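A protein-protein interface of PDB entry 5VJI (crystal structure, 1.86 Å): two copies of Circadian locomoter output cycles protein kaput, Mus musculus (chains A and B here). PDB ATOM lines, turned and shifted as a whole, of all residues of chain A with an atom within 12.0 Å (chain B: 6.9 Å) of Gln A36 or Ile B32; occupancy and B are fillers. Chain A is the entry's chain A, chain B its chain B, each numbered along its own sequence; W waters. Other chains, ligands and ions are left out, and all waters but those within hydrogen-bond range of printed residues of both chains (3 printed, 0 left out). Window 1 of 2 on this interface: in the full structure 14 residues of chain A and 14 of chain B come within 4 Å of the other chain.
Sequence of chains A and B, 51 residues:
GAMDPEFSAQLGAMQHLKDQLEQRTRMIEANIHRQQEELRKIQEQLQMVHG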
ATOM      1  N   THR A  25     -13.135  -4.238  15.649  1.00  0.00           N
ATOM      2  CA  THR A  25     -12.363  -3.384  14.761  1.00  0.00           C
ATOM      3  C   THR A  25     -12.099  -2.031  15.417  1.00  0.00           C
ATOM      4  O   THR A  25     -11.019  -1.467  15.234  1.00  0.00           O
ATOM      5  CB  THR A  25     -13.033  -3.131  13.400  1.00  0.00           C
ATOM      6  OG1 THR A  25     -14.219  -2.335  13.549  1.00  0.00           O
ATOM      7  CG2 THR A  25     -13.263  -4.415  12.552  1.00  0.00           C
ATOM      8  N   ARG A  26     -13.077  -1.490  16.161  1.00  0.00           N
ATOM      9  CA  ARG A  26     -12.843  -0.239  16.895  1.00  0.00           C
ATOM     10  C   ARG A  26     -11.698  -0.397  17.883  1.00  0.00           C
ATOM     11  O   ARG A  26     -10.889   0.511  18.038  1.00  0.00           O
ATOM     12  CB  ARG A  26     -14.096   0.220  17.660  1.00  0.00           C
ATOM     13  CG  ARG A  26     -15.175   0.748  16.784  1.00  0.00           C
ATOM     14  CD  ARG A  26     -16.418   1.272  17.506  1.00  0.00           C
ATOM     15  NE  ARG A  26     -17.502   1.368  16.524  1.00  0.00           N
ATOM     16  CZ  ARG A  26     -18.556   0.560  16.502  1.00  0.00           C
ATOM     17  NH1 ARG A  26     -19.479   0.691  15.548  1.00  0.00           N
ATOM     18  NH2 ARG A  26     -18.698  -0.367  17.455  1.00  0.00           N
ATOM     19  N   MET A  27     -11.632  -1.530  18.573  1.00  0.00           N
ATOM     20  CA  MET A  27     -10.555  -1.840  19.531  1.00  0.00           C
ATOM     21  C   MET A  27      -9.152  -1.888  18.864  1.00  0.00           C
ATOM     22  O   MET A  27      -8.161  -1.352  19.401  1.00  0.00           O
ATOM     23  CB  MET A  27     -10.830  -3.197  20.202  1.00  0.00           C
ATOM     24  CG  MET A  27     -10.703  -3.271  21.702  1.00  0.00           C
ATOM     25  SD  MET A  27     -11.605  -4.928  22.390  1.00  0.00           S
ATOM     26  CE  MET A  27     -13.447  -4.518  21.879  1.00  0.00           C
ATOM     27  N   ILE A  28      -9.095  -2.599  17.740  1.00  0.00           N
ATOM     28  CA  ILE A  28      -7.891  -2.659  16.903  1.00  0.00           C
ATOM     29  C   ILE A  28      -7.491  -1.253  16.476  1.00  0.00           C
ATOM     30  O   ILE A  28      -6.332  -0.862  16.624  1.00  0.00           O
ATOM     31  CB  ILE A  28      -8.100  -3.549  15.663  1.00  0.00           C
ATOM     32  CG1 ILE A  28      -8.401  -4.999  16.055  1.00  0.00           C
ATOM     33  CG2 ILE A  28      -6.805  -3.477  14.702  1.00  0.00           C
ATOM     34  CD1 ILE A  28      -8.974  -5.846  14.841  1.00  0.00           C
ATOM     35  N   GLU A  29      -8.468  -0.459  16.002  1.00  0.00           N
ATOM     36  CA  GLU A  29      -8.147   0.892  15.533  1.00  0.00           C
ATOM     37  C   GLU A  29      -7.502   1.714  16.651  1.00  0.00           C
ATOM     38  O   GLU A  29      -6.491   2.384  16.424  1.00  0.00           O
ATOM     39  CB  GLU A  29      -9.416   1.581  15.011  1.00  0.00           C
ATOM     40  CG  GLU A  29      -9.132   2.891  14.247  1.00  0.00           C
ATOM     41  CD  GLU A  29     -10.384   3.363  13.519  1.00  0.00           C
ATOM     42  OE1 GLU A  29     -11.415   2.643  13.592  1.00  0.00           O
ATOM     43  OE2 GLU A  29     -10.360   4.435  12.880  1.00  0.00           O
ATOM     44  N   ALA A  30      -8.049   1.631  17.869  1.00  0.00           N
ATOM     45  CA  ALA A  30      -7.545   2.392  19.020  1.00  0.00           C
ATOM     46  C   ALA A  30      -6.176   1.877  19.463  1.00  0.00           C
ATOM     47  O   ALA A  30      -5.310   2.682  19.800  1.00  0.00           O
ATOM     48  CB  ALA A  30      -8.539   2.365  20.183  1.00  0.00           C
ATOM     49  N   ASN A  31      -5.952   0.560  19.447  1.00  0.00           N
ATOM     50  CA  ASN A  31      -4.640  -0.002  19.759  1.00  0.00           C
ATOM     51  C   ASN A  31      -3.580   0.434  18.771  1.00  0.00           C
ATOM     52  O   ASN A  31      -2.429   0.682  19.161  1.00  0.00           O
ATOM     53  CB  ASN A  31      -4.662  -1.518  19.710  1.00  0.00           C
ATOM     54  CG  ASN A  31      -5.018  -2.140  21.006  1.00  0.00           C
ATOM     55  OD1 ASN A  31      -4.529  -1.734  22.061  1.00  0.00           O
ATOM     56  ND2 ASN A  31      -5.814  -3.204  20.939  1.00  0.00           N
ATOM     57  N   ILE A  32      -3.925   0.445  17.477  1.00  0.00           N
ATOM     58  CA  ILE A  32      -2.967   0.902  16.473  1.00  0.00           C
ATOM     59  C   ILE A  32      -2.551   2.334  16.779  1.00  0.00           C
ATOM     60  O   ILE A  32      -1.372   2.696  16.674  1.00  0.00           O
ATOM     61  CB  ILE A  32      -3.568   0.768  15.059  1.00  0.00           C
ATOM     62  CG1 ILE A  32      -3.543  -0.704  14.606  1.00  0.00           C
ATOM     63  CG2 ILE A  32      -2.866   1.735  14.062  1.00  0.00           C
ATOM     64  CD1 ILE A  32      -4.200  -0.915  13.264  1.00  0.00           C
ATOM     65  N   HIS A  33      -3.513   3.183  17.123  1.00  0.00           N
ATOM     66  CA  HIS A  33      -3.154   4.563  17.441  1.00  0.00           C
ATOM     67  C   HIS A  33      -2.239   4.624  18.659  1.00  0.00           C
ATOM     68  O   HIS A  33      -1.308   5.431  18.684  1.00  0.00           O
ATOM     69  CB  HIS A  33      -4.421   5.387  17.652  1.00  0.00           C
ATOM     70  CG  HIS A  33      -5.109   5.744  16.379  1.00  0.00           C
ATOM     71  ND1 HIS A  33      -6.464   5.578  16.190  1.00  0.00           N
ATOM     72  CD2 HIS A  33      -4.623   6.251  15.221  1.00  0.00           C
ATOM     73  CE1 HIS A  33      -6.784   5.967  14.969  1.00  0.00           C
ATOM     74  NE2 HIS A  33      -5.686   6.382  14.363  1.00  0.00           N
ATOM     75  N   ARG A  34      -2.515   3.807  19.687  1.00  0.00           N
ATOM     76  CA  ARG A  34      -1.653   3.797  20.868  1.00  0.00           C
ATOM     77  C   ARG A  34      -0.262   3.281  20.531  1.00  0.00           C
ATOM     78  O   ARG A  34       0.735   3.807  21.045  1.00  0.00           O
ATOM     79  CB  ARG A  34      -2.300   2.946  21.966  1.00  0.00           C
ATOM     80  CG  ARG A  34      -1.668   3.061  23.335  1.00  0.00           C
ATOM     81  CD  ARG A  34      -2.409   2.212  24.376  1.00  0.00           C
ATOM     82  NE  ARG A  34      -2.727   0.866  23.890  1.00  0.00           N
ATOM     83  CZ  ARG A  34      -1.847  -0.099  23.614  1.00  0.00           C
ATOM     84  NH1 ARG A  34      -0.547   0.102  23.741  1.00  0.00           N
ATOM     85  NH2 ARG A  34      -2.284  -1.272  23.163  1.00  0.00           N
ATOM     86  N   GLN A  35      -0.167   2.243  19.684  1.00  0.00           N
ATOM     87  CA  GLN A  35       1.146   1.704  19.327  1.00  0.00           C
ATOM     88  C   GLN A  35       1.941   2.713  18.512  1.00  0.00           C
ATOM     89  O   GLN A  35       3.156   2.828  18.653  1.00  0.00           O
ATOM     90  CB  GLN A  35       0.973   0.403  18.526  1.00  0.00           C
ATOM     91  CG  GLN A  35       0.415  -0.743  19.369  1.00  0.00           C
ATOM     92  CD  GLN A  35      -0.088  -1.857  18.462  1.00  0.00           C
ATOM     93  OE1 GLN A  35      -0.350  -1.630  17.275  1.00  0.00           O
ATOM     94  NE2 GLN A  35      -0.232  -3.052  19.010  1.00  0.00           N
ATOM     95  N   GLN A  36       1.267   3.471  17.661  1.00  0.00           N
ATOM     96  CA  GLN A  36       1.960   4.556  16.971  1.00  0.00           C
ATOM     97  C   GLN A  36       2.530   5.585  17.942  1.00  0.00           C
ATOM     98  O   GLN A  36       3.639   6.090  17.729  1.00  0.00           O
ATOM     99  CB  GLN A  36       1.014   5.230  15.969  1.00  0.00           C
ATOM    100  CG  GLN A  36       1.038   4.527  14.615  1.00  0.00           C
ATOM    101  CD  GLN A  36      -0.144   4.866  13.698  1.00  0.00           C
ATOM    102  OE1 GLN A  36      -1.079   5.598  14.070  1.00  0.00           O
ATOM    103  NE2 GLN A  36      -0.130   4.286  12.505  1.00  0.00           N
ATOM    104  N   GLU A  37       1.788   5.930  18.996  1.00  0.00           N
ATOM    105  CA  GLU A  37       2.304   6.884  19.976  1.00  0.00           C
ATOM    106  C   GLU A  37       3.484   6.288  20.756  1.00  0.00           C
ATOM    107  O   GLU A  37       4.446   7.007  21.087  1.00  0.00           O
ATOM    108  CB  GLU A  37       1.174   7.315  20.934  1.00  0.00           C
ATOM    109  CG  GLU A  37       1.633   8.222  22.102  1.00  0.00           C
ATOM    110  CD  GLU A  37       2.530   9.397  21.660  1.00  0.00           C
ATOM    111  OE1 GLU A  37       2.245  10.028  20.610  1.00  0.00           O
ATOM    112  OE2 GLU A  37       3.522   9.693  22.371  1.00  0.00           O
ATOM    113  N   GLU A  38       3.443   4.980  21.056  1.00  0.00           N
ATOM    114  CA  GLU A  38       4.588   4.314  21.698  1.00  0.00           C
ATOM    115  C   GLU A  38       5.834   4.327  20.818  1.00  0.00           C
ATOM    116  O   GLU A  38       6.961   4.522  21.323  1.00  0.00           O
ATOM    117  CB  GLU A  38       4.246   2.868  22.078  1.00  0.00           C
ATOM    118  CG  GLU A  38       3.177   2.771  23.157  1.00  0.00           C
ATOM    119  CD  GLU A  38       2.531   1.382  23.257  1.00  0.00           C
ATOM    120  OE1 GLU A  38       3.168   0.366  22.919  1.00  0.00           O
ATOM    121  OE2 GLU A  38       1.350   1.312  23.652  1.00  0.00           O
ATOM    122  N   LEU A  39       5.674   4.111  19.512  1.00  0.00           N
ATOM    123  CA  LEU A  39       6.846   4.194  18.630  1.00  0.00           C
ATOM    124  C   LEU A  39       7.393   5.614  18.611  1.00  0.00           C
ATOM    125  O   LEU A  39       8.600   5.815  18.631  1.00  0.00           O
ATOM    126  CB  LEU A  39       6.505   3.764  17.199  1.00  0.00           C
ATOM    127  CG  LEU A  39       6.304   2.283  17.020  1.00  0.00           C
ATOM    128  CD1 LEU A  39       5.572   1.996  15.697  1.00  0.00           C
ATOM    129  CD2 LEU A  39       7.661   1.671  17.014  1.00  0.00           C
ATOM    130  N   ARG A  40       6.503   6.607  18.543  1.00  0.00           N
ATOM    131  CA  ARG A  40       6.923   8.003  18.627  1.00  0.00           C
ATOM    132  C   ARG A  40       7.774   8.261  19.864  1.00  0.00           C
ATOM    133  O   ARG A  40       8.830   8.912  19.778  1.00  0.00           O
ATOM    134  CB  ARG A  40       5.693   8.905  18.636  1.00  0.00           C
ATOM    135  CG  ARG A  40       5.936  10.290  18.055  1.00  0.00           C
ATOM    136  CD  ARG A  40       4.902  11.287  18.565  1.00  0.00           C
ATOM    137  NE  ARG A  40       5.370  11.966  19.766  1.00  0.00           N
ATOM    138  CZ  ARG A  40       4.577  12.624  20.606  1.00  0.00           C
ATOM    139  NH1 ARG A  40       3.271  12.682  20.373  1.00  0.00           N
ATOM    140  NH2 ARG A  40       5.086  13.224  21.675  1.00  0.00           N
ATOM    141  N   LYS A  41       7.308   7.805  21.035  1.00  0.00           N
ATOM    142  CA  LYS A  41       8.053   7.993  22.277  1.00  0.00           C
ATOM    143  C   LYS A  41       9.446   7.357  22.213  1.00  0.00           C
ATOM    144  O   LYS A  41      10.412   7.928  22.711  1.00  0.00           O
ATOM    145  CB  LYS A  41       7.285   7.389  23.462  1.00  0.00           C
ATOM    146  CG  LYS A  41       6.201   8.279  24.054  1.00  0.00           C
ATOM    147  CD  LYS A  41       5.899   7.883  25.501  1.00  0.00           C
ATOM    148  CE  LYS A  41       4.617   7.087  25.627  1.00  0.00           C
ATOM    149  NZ  LYS A  41       3.426   7.955  25.372  1.00  0.00           N
ATOM    150  N   ILE A  42       9.546   6.142  21.673  1.00  0.00           N
ATOM    151  CA  ILE A  42      10.835   5.475  21.544  1.00  0.00           C
ATOM    152  C   ILE A  42      11.758   6.273  20.627  1.00  0.00           C
ATOM    153  O   ILE A  42      12.948   6.409  20.905  1.00  0.00           O
ATOM    154  CB  ILE A  42      10.648   4.038  21.017  1.00  0.00           C
ATOM    155  CG1 ILE A  42       9.934   3.159  22.043  1.00  0.00           C
ATOM    156  CG2 ILE A  42      12.015   3.449  20.553  1.00  0.00           C
ATOM    157  CD1 ILE A  42       9.391   1.856  21.410  1.00  0.00           C
ATOM    158  N   GLN A  43      11.222   6.780  19.500  1.00  0.00           N
ATOM    159  CA  GLN A  43      12.043   7.559  18.577  1.00  0.00           C
ATOM    160  C   GLN A  43      12.553   8.829  19.268  1.00  0.00           C
ATOM    161  O   GLN A  43      13.727   9.190  19.148  1.00  0.00           O
ATOM    162  CB  GLN A  43      11.224   7.876  17.302  1.00  0.00           C
ATOM    163  CG  GLN A  43      11.073   6.649  16.407  1.00  0.00           C
ATOM    164  CD  GLN A  43      10.222   6.888  15.166  1.00  0.00           C
ATOM    165  OE1 GLN A  43       9.485   7.875  15.084  1.00  0.00           O
ATOM    166  NE2 GLN A  43      10.302   5.963  14.207  1.00  0.00           N
ATOM    167  N   GLU A  44      11.697   9.472  20.066  1.00  0.00           N
ATOM    168  CA  GLU A  44      12.069  10.708  20.759  1.00  0.00           C
ATOM    169  C   GLU A  44      13.198  10.466  21.763  1.00  0.00           C
ATOM    170  O   GLU A  44      14.132  11.272  21.871  1.00  0.00           O
ATOM    171  CB  GLU A  44      10.831  11.261  21.477  1.00  0.00           C
ATOM    172  CG  GLU A  44      10.587  12.767  21.432  1.00  0.00           C
ATOM    173  CD  GLU A  44       9.115  13.116  21.780  1.00  0.00           C
ATOM    174  OE1 GLU A  44       8.569  12.538  22.751  1.00  0.00           O
ATOM    175  OE2 GLU A  44       8.499  13.942  21.065  1.00  0.00           O
ATOM    176  N   GLN A  45      13.114   9.365  22.508  1.00  0.00           N
ATOM    177  CA  GLN A  45      14.157   8.970  23.463  1.00  0.00           C
ATOM    178  C   GLN A  45      15.495   8.695  22.770  1.00  0.00           C
ATOM    179  O   GLN A  45      16.559   9.087  23.274  1.00  0.00           O
ATOM    180  CB  GLN A  45      13.692   7.724  24.244  1.00  0.00           C
ATOM    181  CG  GLN A  45      12.543   7.993  25.174  1.00  0.00           C
ATOM    182  CD  GLN A  45      12.528   7.079  26.392  1.00  0.00           C
ATOM    183  OE1 GLN A  45      12.677   5.856  26.284  1.00  0.00           O
ATOM    184  NE2 GLN A  45      12.357   7.682  27.568  1.00  0.00           N
ATOM    185  N   MET B  27      10.569  -0.587  11.023  1.00  0.00           N
ATOM    186  CA  MET B  27      10.032  -1.877  10.636  1.00  0.00           C
ATOM    187  C   MET B  27       8.671  -2.053  11.278  1.00  0.00           C
ATOM    188  O   MET B  27       7.744  -2.473  10.632  1.00  0.00           O
ATOM    189  CB  MET B  27      10.927  -3.064  11.111  1.00  0.00           C
ATOM    190  CG  MET B  27      12.328  -3.201  10.548  1.00  0.00           C
ATOM    191  SD  MET B  27      13.351  -4.647  11.479  1.00  0.00           S
ATOM    192  CE  MET B  27      12.111  -6.143  11.206  1.00  0.00           C
ATOM    193  N   ILE B  28       8.582  -1.799  12.581  1.00  0.00           N
ATOM    194  CA  ILE B  28       7.301  -1.965  13.260  1.00  0.00           C
ATOM    195  C   ILE B  28       6.257  -0.988  12.704  1.00  0.00           C
ATOM    196  O   ILE B  28       5.094  -1.362  12.478  1.00  0.00           O
ATOM    197  CB  ILE B  28       7.492  -1.821  14.775  1.00  0.00           C
ATOM    198  CG1 ILE B  28       8.354  -2.981  15.301  1.00  0.00           C
ATOM    199  CG2 ILE B  28       6.158  -1.819  15.457  1.00  0.00           C
ATOM    200  CD1 ILE B  28       8.793  -2.828  16.803  1.00  0.00           C
ATOM    201  N   GLU B  29       6.665   0.255  12.427  1.00  0.00           N
ATOM    202  CA  GLU B  29       5.766   1.229  11.794  1.00  0.00           C
ATOM    203  C   GLU B  29       5.221   0.724  10.471  1.00  0.00           C
ATOM    204  O   GLU B  29       4.041   0.953  10.152  1.00  0.00           O
ATOM    205  CB  GLU B  29       6.486   2.567  11.542  1.00  0.00           C
ATOM    206  CG  GLU B  29       6.514   3.521  12.736  1.00  0.00           C
ATOM    207  CD  GLU B  29       7.209   4.850  12.443  1.00  0.00           C
ATOM    208  OE1 GLU B  29       7.986   4.933  11.460  1.00  0.00           O
ATOM    209  OE2 GLU B  29       6.970   5.812  13.210  1.00  0.00           O
ATOM    210  N   ALA B  30       6.067   0.080   9.652  1.00  0.00           N
ATOM    211  CA  ALA B  30       5.550  -0.397   8.362  1.00  0.00           C
ATOM    212  C   ALA B  30       4.554  -1.544   8.553  1.00  0.00           C
ATOM    213  O   ALA B  30       3.531  -1.610   7.851  1.00  0.00           O
ATOM    214  CB  ALA B  30       6.696  -0.829   7.428  1.00  0.00           C
ATOM    215  N   ASN B  31       4.825  -2.451   9.500  1.00  0.00           N
ATOM    216  CA  ASN B  31       3.857  -3.495   9.814  1.00  0.00           C
ATOM    217  C   ASN B  31       2.522  -2.898  10.274  1.00  0.00           C
ATOM    218  O   ASN B  31       1.449  -3.384   9.886  1.00  0.00           O
ATOM    219  CB  ASN B  31       4.396  -4.445  10.893  1.00  0.00           C
ATOM    220  CG  ASN B  31       5.697  -5.143  10.500  1.00  0.00           C
ATOM    221  OD1 ASN B  31       6.084  -5.174   9.324  1.00  0.00           O
ATOM    222  ND2 ASN B  31       6.371  -5.732  11.494  1.00  0.00           N
ATOM    223  N   ILE B  32       2.556  -1.866  11.122  1.00  0.00           N
ATOM    224  CA  ILE B  32       1.284  -1.278  11.576  1.00  0.00           C
ATOM    225  C   ILE B  32       0.547  -0.590  10.425  1.00  0.00           C
ATOM    226  O   ILE B  32      -0.693  -0.627  10.333  1.00  0.00           O
ATOM    227  CB  ILE B  32       1.599  -0.304  12.731  1.00  0.00           C
ATOM    228  CG1 ILE B  32       2.056  -1.108  13.956  1.00  0.00           C
ATOM    229  CG2 ILE B  32       0.371   0.521  13.111  1.00  0.00           C
ATOM    230  CD1 ILE B  32       2.590  -0.233  15.075  1.00  0.00           C
ATOM    231  N   HIS B  33       1.292   0.015   9.498  1.00  0.00           N
ATOM    232  CA  HIS B  33       0.642   0.644   8.354  1.00  0.00           C
ATOM    233  C   HIS B  33      -0.119  -0.384   7.545  1.00  0.00           C
ATOM    234  O   HIS B  33      -1.224  -0.112   7.068  1.00  0.00           O
ATOM    235  CB  HIS B  33       1.680   1.364   7.468  1.00  0.00           C
ATOM    236  CG  HIS B  33       1.074   2.410   6.576  1.00  0.00           C
ATOM    237  ND1 HIS B  33       0.770   2.184   5.250  1.00  0.00           N
ATOM    238  CD2 HIS B  33       0.674   3.679   6.840  1.00  0.00           C
ATOM    239  CE1 HIS B  33       0.226   3.273   4.731  1.00  0.00           C
ATOM    240  NE2 HIS B  33       0.155   4.193   5.676  1.00  0.00           N
ATOM    241  N   ARG B  34       0.449  -1.585   7.396  1.00  0.00           N
ATOM    242  CA  ARG B  34      -0.212  -2.654   6.652  1.00  0.00           C
ATOM    243  C   ARG B  34      -1.438  -3.154   7.392  1.00  0.00           C
ATOM    244  O   ARG B  34      -2.449  -3.505   6.780  1.00  0.00           O
ATOM    245  CB  ARG B  34       0.755  -3.819   6.432  1.00  0.00           C
ATOM    246  CG  ARG B  34       1.730  -3.578   5.275  1.00  0.00           C
ATOM    247  CD  ARG B  34       2.625  -4.795   4.966  1.00  0.00           C
ATOM    248  NE  ARG B  34       3.689  -5.020   5.957  1.00  0.00           N
ATOM    249  CZ  ARG B  34       4.885  -4.415   5.954  1.00  0.00           C
ATOM    250  NH1 ARG B  34       5.179  -3.517   5.019  1.00  0.00           N
ATOM    251  NH2 ARG B  34       5.788  -4.700   6.900  1.00  0.00           N
ATOM    252  N   GLN B  35      -1.359  -3.205   8.719  1.00  0.00           N
ATOM    253  CA  GLN B  35      -2.515  -3.583   9.527  1.00  0.00           C
ATOM    254  C   GLN B  35      -3.630  -2.560   9.412  1.00  0.00           C
ATOM    255  O   GLN B  35      -4.819  -2.901   9.448  1.00  0.00           O
ATOM    256  CB  GLN B  35      -2.111  -3.687  10.985  1.00  0.00           C
ATOM    257  CG  GLN B  35      -1.208  -4.918  11.335  1.00  0.00           C
ATOM    258  CD  GLN B  35      -0.767  -4.863  12.788  1.00  0.00           C
ATOM    259  OE1 GLN B  35      -1.496  -4.369  13.627  1.00  0.00           O
ATOM    260  NE2 GLN B  35       0.452  -5.277  13.061  1.00  0.00           N
ATOM    261  N   GLN B  36      -3.261  -1.294   9.383  1.00  0.00           N
ATOM    262  CA  GLN B  36      -4.279  -0.259   9.233  1.00  0.00           C
ATOM    263  C   GLN B  36      -5.017  -0.391   7.909  1.00  0.00           C
ATOM    264  O   GLN B  36      -6.207  -0.093   7.836  1.00  0.00           O
ATOM    265  CB  GLN B  36      -3.631   1.117   9.324  1.00  0.00           C
ATOM    266  CG  GLN B  36      -3.674   1.753  10.654  1.00  0.00           C
ATOM    267  CD  GLN B  36      -3.078   3.165  10.578  1.00  0.00           C
ATOM    268  OE1 GLN B  36      -1.990   3.351  10.027  1.00  0.00           O
ATOM    269  NE2 GLN B  36      -3.799   4.149  11.085  1.00  0.00           N
ATOM    270  N   GLU B  37      -4.310  -0.766   6.829  1.00  0.00           N
ATOM    271  CA  GLU B  37      -4.986  -0.962   5.546  1.00  0.00           C
ATOM    272  C   GLU B  37      -5.896  -2.193   5.578  1.00  0.00           C
ATOM    273  O   GLU B  37      -6.990  -2.192   4.983  1.00  0.00           O
ATOM    274  CB  GLU B  37      -3.950  -1.081   4.420  1.00  0.00           C
ATOM    275  CG  GLU B  37      -4.532  -1.303   3.037  1.00  0.00           C
ATOM    276  CD  GLU B  37      -5.587  -0.274   2.661  1.00  0.00           C
ATOM    277  OE1 GLU B  37      -5.429   0.914   3.028  1.00  0.00           O
ATOM    278  OE2 GLU B  37      -6.580  -0.659   2.001  1.00  0.00           O
ATOM    279  N   GLU B  38      -5.469  -3.263   6.251  1.00  0.00           N
ATOM    280  CA  GLU B  38      -6.372  -4.412   6.371  1.00  0.00           C
ATOM    281  C   GLU B  38      -7.599  -4.068   7.227  1.00  0.00           C
ATOM    282  O   GLU B  38      -8.723  -4.554   6.977  1.00  0.00           O
ATOM    283  CB  GLU B  38      -5.616  -5.579   6.980  1.00  0.00           C
ATOM    284  CG  GLU B  38      -6.440  -6.825   7.172  1.00  0.00           C
ATOM    285  CD  GLU B  38      -6.994  -7.362   5.850  1.00  0.00           C
ATOM    286  OE1 GLU B  38      -6.233  -7.407   4.844  1.00  0.00           O
ATOM    287  OE2 GLU B  38      -8.191  -7.725   5.827  1.00  0.00           O
HETATM  288  O   HOH W   1      -2.293   6.306  11.474  1.00  0.00           O
HETATM  289  O   HOH W   2       7.663   8.516  12.413  1.00  0.00           O
HETATM  290  O   HOH W   3       4.465   6.069  14.602  1.00  0.00           O
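Water W1 lies within hydrogen-bond range of the side-chain amide nitrogen of Gln B36 (2.7 Å) and the side-chain amide oxygen of Gln A36 (3.0 Å). Water W3 lies within hydrogen-bond range of OE2 of Glu B29 (2.9 Å) and O of Gln A36 (3.2 Å). Water W2 bridges OE2 of Glu B29 (2.9 Å) and OE1 of Gln A43 (3.3 Å).
The side-chain amide nitrogen (NE2) of Gln A36 lies within hydrogen-bond range of the side-chain amide oxygen (OE1) of Gln B36 (3.2 Å). NE2 of Gln A43 sits at hydrogen-bond distance from OE2 of Glu B29 (3.5 Å).
Ile B32 touches its own counterpart, Ile A32. Ile A32 touches Gln B36, and with the chains exchanged Gln A36 touches Ile B32. Gln A35 touches Ile B32, but with the chains exchanged Ile A32 does not touch Gln B35 (4.2 Å). Gln B36 touches its own counterpart, Gln A36. Of the 9 pairs that touch across the chains among the printed residues, 4 have their exchanged pair printed and touching as well.
Ile A32 touches Ile B32. Ile A32 touches Gln B36. CB of Gln A35 touches CD1 of Ile B32, at 3.9 Å. CG2 of Ile B32 touches NE2 of Gln A36, 3.8 Å away. Leu A39 touches Ile B28 (CD1 to CG2, 3.9 Å). CD1 of Leu A39 touches CG of Glu B29 (3.5 Å). Leu A39 touches Ile B32 (CD1 to CD1, 3.8 Å).
Of the 12 printed residues of chain B, 4 touch a printed residue of chain A. Printed residues of chain B that touch a printed residue of chain A: Ile B28, Glu B29, Ile B32 and Gln B36. Of the 21 printed residues of chain A, 5 touch a printed residue of chain B. Among the printed residues, no Asp or Glu carboxylate lies within 4 Å of a Lys or Arg side-chain nitrogen of the other chain.
Gln A36 touches two residues of chain B. Ile B32 touches just these residues of chain A: Ile A32 (3.6 Å), Gln A35 (3.9 Å), Gln A36 (3.8 Å) and Leu A39 (3.8 Å). Of the printed residues of chain A, Ile B28 touches Leu A39 (3.9 Å). Glu B29 touches two residues of chain A. Ala B30 touches none of the printed residues of chain A. No residue of chain A comes within 4 Å of Asn B31. Arg B34 touches none of the printed residues of chain A. No residue of chain A comes within 4 Å of Gln B35. Of the printed residues of chain B, Ile A32 touches Ile B32 and Gln B36. Of the printed residues of chain B, Gln A43 touches Glu B29. Of the printed residues of chain B, Leu A39 touches Ile B28 (3.9 Å), Glu B29 (3.5 Å) and Ile B32 (3.8 Å). Ala A30 touches none of the printed residues of chain B. Met A27 touches none of the printed residues of chain B.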
